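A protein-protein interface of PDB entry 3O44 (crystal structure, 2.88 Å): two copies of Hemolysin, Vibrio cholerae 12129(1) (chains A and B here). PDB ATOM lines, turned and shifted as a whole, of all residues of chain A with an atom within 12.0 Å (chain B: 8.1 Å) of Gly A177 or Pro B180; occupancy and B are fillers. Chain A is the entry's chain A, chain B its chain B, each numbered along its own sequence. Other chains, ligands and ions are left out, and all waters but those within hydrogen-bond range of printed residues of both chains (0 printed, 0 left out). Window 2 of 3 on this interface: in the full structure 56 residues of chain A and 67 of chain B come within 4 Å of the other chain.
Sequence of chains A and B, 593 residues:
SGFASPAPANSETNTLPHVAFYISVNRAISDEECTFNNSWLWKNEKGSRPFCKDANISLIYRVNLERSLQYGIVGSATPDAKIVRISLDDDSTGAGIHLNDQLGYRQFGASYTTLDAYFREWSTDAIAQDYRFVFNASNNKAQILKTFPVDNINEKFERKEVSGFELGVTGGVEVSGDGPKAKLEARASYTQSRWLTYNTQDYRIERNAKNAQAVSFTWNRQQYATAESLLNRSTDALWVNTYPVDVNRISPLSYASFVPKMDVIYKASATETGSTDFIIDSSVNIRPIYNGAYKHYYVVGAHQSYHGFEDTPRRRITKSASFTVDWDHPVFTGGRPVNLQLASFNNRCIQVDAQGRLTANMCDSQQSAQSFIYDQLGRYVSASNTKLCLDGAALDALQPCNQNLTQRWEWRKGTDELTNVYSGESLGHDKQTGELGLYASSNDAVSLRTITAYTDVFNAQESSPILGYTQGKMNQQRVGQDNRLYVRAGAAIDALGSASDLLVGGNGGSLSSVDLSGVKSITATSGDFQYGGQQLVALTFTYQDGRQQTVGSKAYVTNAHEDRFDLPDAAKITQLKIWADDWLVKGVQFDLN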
ATOM      1  N   VAL A 173      13.801  30.620   3.208  1.00  0.00           N
ATOM      2  CA  VAL A 173      14.542  31.284   4.273  1.00  0.00           C
ATOM      3  C   VAL A 173      14.960  30.260   5.317  1.00  0.00           C
ATOM      4  O   VAL A 173      14.116  29.686   6.008  1.00  0.00           O
ATOM      5  CB  VAL A 173      13.700  32.386   4.950  1.00  0.00           C
ATOM      6  CG1 VAL A 173      14.204  32.682   6.356  1.00  0.00           C
ATOM      7  CG2 VAL A 173      13.697  33.647   4.099  1.00  0.00           C
ATOM      8  N   GLU A 174      16.265  30.022   5.416  1.00  0.00           N
ATOM      9  CA  GLU A 174      16.800  29.104   6.414  1.00  0.00           C
ATOM     10  C   GLU A 174      17.612  29.862   7.454  1.00  0.00           C
ATOM     11  O   GLU A 174      18.447  30.699   7.114  1.00  0.00           O
ATOM     12  CB  GLU A 174      17.670  28.020   5.759  1.00  0.00           C
ATOM     13  CG  GLU A 174      18.221  26.987   6.743  1.00  0.00           C
ATOM     14  CD  GLU A 174      19.169  25.989   6.094  1.00  0.00           C
ATOM     15  OE1 GLU A 174      19.550  26.196   4.915  1.00  0.00           O
ATOM     16  OE2 GLU A 174      19.534  25.000   6.772  1.00  0.00           O
ATOM     17  N   VAL A 175      17.357  29.572   8.725  1.00  0.00           N
ATOM     18  CA  VAL A 175      18.165  30.123   9.803  1.00  0.00           C
ATOM     19  C   VAL A 175      18.801  28.997  10.629  1.00  0.00           C
ATOM     20  O   VAL A 175      18.121  28.066  11.060  1.00  0.00           O
ATOM     21  CB  VAL A 175      17.340  31.047  10.706  1.00  0.00           C
ATOM     22  CG1 VAL A 175      16.462  30.235  11.652  1.00  0.00           C
ATOM     23  CG2 VAL A 175      18.263  31.962  11.481  1.00  0.00           C
ATOM     24  N   SER A 176      20.110  29.077  10.833  1.00  0.00           N
ATOM     25  CA  SER A 176      20.824  28.048  11.584  1.00  0.00           C
ATOM     26  C   SER A 176      21.974  28.658  12.381  1.00  0.00           C
ATOM     27  O   SER A 176      22.235  29.858  12.290  1.00  0.00           O
ATOM     28  CB  SER A 176      21.348  26.959  10.640  1.00  0.00           C
ATOM     29  OG  SER A 176      22.267  27.481   9.690  1.00  0.00           O
ATOM     30  N   GLY A 177      22.655  27.831  13.168  1.00  0.00           N
ATOM     31  CA  GLY A 177      23.849  28.266  13.869  1.00  0.00           C
ATOM     32  C   GLY A 177      24.904  28.769  12.898  1.00  0.00           C
ATOM     33  O   GLY A 177      25.531  29.803  13.138  1.00  0.00           O
ATOM     34  N   ASP A 178      25.090  28.042  11.796  1.00  0.00           N
ATOM     35  CA  ASP A 178      26.071  28.404  10.773  1.00  0.00           C
ATOM     36  C   ASP A 178      25.810  29.786  10.153  1.00  0.00           C
ATOM     37  O   ASP A 178      26.747  30.479   9.754  1.00  0.00           O
ATOM     38  CB  ASP A 178      26.143  27.327   9.684  1.00  0.00           C
ATOM     39  N   GLY A 179      24.543  30.184  10.079  1.00  0.00           N
ATOM     40  CA  GLY A 179      24.172  31.476   9.519  1.00  0.00           C
ATOM     41  C   GLY A 179      22.843  31.455   8.784  1.00  0.00           C
ATOM     42  O   GLY A 179      22.245  30.394   8.610  1.00  0.00           O
ATOM     43  N   PRO A 180      22.359  32.633   8.364  1.00  0.00           N
ATOM     44  CA  PRO A 180      21.114  32.761   7.595  1.00  0.00           C
ATOM     45  C   PRO A 180      21.300  32.600   6.080  1.00  0.00           C
ATOM     46  O   PRO A 180      22.097  33.333   5.484  1.00  0.00           O
ATOM     47  CB  PRO A 180      20.658  34.195   7.903  1.00  0.00           C
ATOM     48  CG  PRO A 180      21.467  34.621   9.090  1.00  0.00           C
ATOM     49  CD  PRO A 180      22.773  33.921   8.930  1.00  0.00           C
ATOM     50  N   LYS A 181      20.558  31.663   5.482  1.00  0.00           N
ATOM     51  CA  LYS A 181      20.539  31.456   4.029  1.00  0.00           C
ATOM     52  C   LYS A 181      19.172  31.848   3.435  1.00  0.00           C
ATOM     53  O   LYS A 181      18.176  31.962   4.156  1.00  0.00           O
ATOM     54  CB  LYS A 181      20.884  29.997   3.681  1.00  0.00           C
ATOM     55  N   VAL B 173      12.451  21.742  10.379  1.00  0.00           N
ATOM     56  CA  VAL B 173      13.249  21.740  11.602  1.00  0.00           C
ATOM     57  C   VAL B 173      14.214  20.558  11.571  1.00  0.00           C
ATOM     58  O   VAL B 173      13.791  19.399  11.633  1.00  0.00           O
ATOM     59  CB  VAL B 173      12.365  21.651  12.869  1.00  0.00           C
ATOM     60  CG1 VAL B 173      13.160  21.123  14.045  1.00  0.00           C
ATOM     61  CG2 VAL B 173      11.760  22.998  13.183  1.00  0.00           C
ATOM     62  N   GLU B 174      15.506  20.848  11.452  1.00  0.00           N
ATOM     63  CA  GLU B 174      16.523  19.808  11.470  1.00  0.00           C
ATOM     64  C   GLU B 174      17.368  19.913  12.736  1.00  0.00           C
ATOM     65  O   GLU B 174      17.816  20.996  13.095  1.00  0.00           O
ATOM     66  CB  GLU B 174      17.418  19.898  10.229  1.00  0.00           C
ATOM     67  CG  GLU B 174      18.478  18.795  10.162  1.00  0.00           C
ATOM     68  CD  GLU B 174      19.447  18.957   8.994  1.00  0.00           C
ATOM     69  OE1 GLU B 174      19.395  20.014   8.324  1.00  0.00           O
ATOM     70  OE2 GLU B 174      20.262  18.027   8.753  1.00  0.00           O
ATOM     71  N   VAL B 175      17.572  18.789  13.417  1.00  0.00           N
ATOM     72  CA  VAL B 175      18.472  18.742  14.566  1.00  0.00           C
ATOM     73  C   VAL B 175      19.590  17.731  14.316  1.00  0.00           C
ATOM     74  O   VAL B 175      19.333  16.584  13.953  1.00  0.00           O
ATOM     75  CB  VAL B 175      17.726  18.400  15.876  1.00  0.00           C
ATOM     76  CG1 VAL B 175      17.411  16.918  15.951  1.00  0.00           C
ATOM     77  CG2 VAL B 175      18.550  18.819  17.078  1.00  0.00           C
ATOM     78  N   SER B 176      20.833  18.165  14.491  1.00  0.00           N
ATOM     79  CA  SER B 176      21.988  17.298  14.258  1.00  0.00           C
ATOM     80  C   SER B 176      23.116  17.595  15.247  1.00  0.00           C
ATOM     81  O   SER B 176      23.015  18.511  16.066  1.00  0.00           O
ATOM     82  CB  SER B 176      22.496  17.428  12.806  1.00  0.00           C
ATOM     83  OG  SER B 176      22.925  18.749  12.505  1.00  0.00           O
ATOM     84  N   GLY B 177      24.182  16.806  15.172  1.00  0.00           N
ATOM     85  CA  GLY B 177      25.364  17.068  15.969  1.00  0.00           C
ATOM     86  C   GLY B 177      25.919  18.448  15.665  1.00  0.00           C
ATOM     87  O   GLY B 177      26.291  19.188  16.579  1.00  0.00           O
ATOM     88  N   ASP B 178      25.963  18.794  14.378  1.00  0.00           N
ATOM     89  CA  ASP B 178      26.488  20.088  13.935  1.00  0.00           C
ATOM     90  C   ASP B 178      25.703  21.271  14.515  1.00  0.00           C
ATOM     91  O   ASP B 178      26.268  22.340  14.739  1.00  0.00           O
ATOM     92  CB  ASP B 178      26.529  20.169  12.404  1.00  0.00           C
ATOM     93  N   GLY B 179      24.410  21.075  14.767  1.00  0.00           N
ATOM     94  CA  GLY B 179      23.562  22.119  15.323  1.00  0.00           C
ATOM     95  C   GLY B 179      22.136  22.069  14.799  1.00  0.00           C
ATOM     96  O   GLY B 179      21.828  21.287  13.900  1.00  0.00           O
ATOM     97  N   PRO B 180      21.245  22.893  15.376  1.00  0.00           N
ATOM     98  CA  PRO B 180      19.845  23.018  14.934  1.00  0.00           C
ATOM     99  C   PRO B 180      19.627  24.004  13.763  1.00  0.00           C
ATOM    100  O   PRO B 180      19.993  25.177  13.860  1.00  0.00           O
ATOM    101  CB  PRO B 180      19.121  23.531  16.195  1.00  0.00           C
ATOM    102  CG  PRO B 180      20.085  23.304  17.326  1.00  0.00           C
ATOM    103  CD  PRO B 180      21.439  23.470  16.713  1.00  0.00           C
ATOM    104  N   LYS B 181      19.028  23.516  12.674  1.00  0.00           N
ATOM    105  CA  LYS B 181      18.657  24.352  11.531  1.00  0.00           C
ATOM    106  C   LYS B 181      17.129  24.463  11.416  1.00  0.00           C
ATOM    107  O   LYS B 181      16.397  23.669  12.010  1.00  0.00           O
ATOM    108  CB  LYS B 181      19.253  23.789  10.237  1.00  0.00           C
ATOM    109  N   ALA B 182      16.649  25.449  10.661  1.00  0.00           N
ATOM    110  CA  ALA B 182      15.203  25.668  10.506  1.00  0.00           C
ATOM    111  C   ALA B 182      14.850  26.453   9.237  1.00  0.00           C
ATOM    112  O   ALA B 182      15.414  27.518   8.982  1.00  0.00           O
ATOM    113  CB  ALA B 182      14.634  26.366  11.732  1.00  0.00           C
ATOM    114  N   LYS B 183      13.905  25.932   8.456  1.00  0.00           N
ATOM    115  CA  LYS B 183      13.544  26.539   7.174  1.00  0.00           C
ATOM    116  C   LYS B 183      12.049  26.873   7.089  1.00  0.00           C
ATOM    117  O   LYS B 183      11.211  26.052   7.456  1.00  0.00           O
ATOM    118  CB  LYS B 183      13.949  25.612   6.015  1.00  0.00           C
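N of Val A175 sits at hydrogen-bond distance from O of Ala B182, at 2.8 Å.
The backbone carbonyl oxygen (O) of Glu B174 is in hydrogen-bond range of the backbone NH (N) of Lys B181, at 2.8 Å. The backbone carbonyl oxygen of Gly A179 sits at hydrogen-bond distance from the side-chain hydroxyl of Ser A176, 3.1 Å away. O of Glu A174 lies within hydrogen-bond range of N of Lys A181, 2.8 Å away.
Glu A174 touches Lys B181, but with the chains exchanged Lys A181 does not touch Glu B174 (11.1 Å). Ser A176 touches Pro B180, but with the chains exchanged Pro A180 does not touch Ser B176 (14.5 Å). Ser A176 touches Lys B181, but with the chains exchanged Lys A181 does not touch Ser B176 (14.4 Å). Gly A177 touches Pro B180, but with the chains exchanged Pro A180 does not touch Gly B177 (16.2 Å). Positions printed for both chains: 173, 174, 175, 176, 177, 178, 179, 180 and 181. Of the 9 pairs that touch across the chains among the printed residues, none has its exchanged pair printed and touching as well.
Of the 9 printed residues of chain A, 5 touch a printed residue of chain B. Along chain A the printed residues that touch a printed residue of chain B span positions 173 to 177. Of the 11 printed residues of chain B, 4 touch a printed residue of chain A. Hydrophobic or aromatic side chains of chain B within 4 Å of the printed part of chain A: Ala B182. Among the printed residues, 9 pairs touch across the chains.
O of Ala B182 touches O of Val A173, at 3.9 Å. O of Val A173 touches CA of Lys B183, at 3.4 Å. OE2 of Glu A174 touches CB of Lys B181, at 3.7 Å. Glu A174 touches Ala B182 (CA to O, 3.3 Å). Val A175 touches Lys B181 (O to C, 3.8 Å). O of Pro B180 touches CA of Ser A176, at 3.8 Å. Ser A176 touches Lys B181. Pro B180 touches Gly A177.
Of the printed residues of chain B, Val A173 touches Ala B182 (3.9 Å) and Lys B183 (3.4 Å). Printed residues of chain B within 4 Å of Glu A174: Lys B181 and Ala B182. Printed residues of chain B within 4 Å of Val A175: Lys B181 and Ala B182. Ser A176 touches just these residues of chain B: Pro B180 and Lys B181. Of chain B, only Pro B180 (3.8 Å) comes within 4 Å of Gly A177. Gly A179 touches none of the printed residues of chain B. Lys A181 touches none of the printed residues of chain B. No residue of chain A comes within 4 Å of Glu B174. No residue of chain A comes within 4 Å of Val B175. No residue of chain A comes within 4 Å of Asp B178. No residue of chain A comes within 4 Å of Gly B179. Pro B180 touches two residues of chain A. Of the printed residues of chain A, Ala B182 touches Val A173, Glu A174 and Val A175. Of the printed residues of chain A, Lys B183 touches Val A173. The nearest residue of chain B that does not touch Gly A177 is Lys B181 (5.5 Å).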
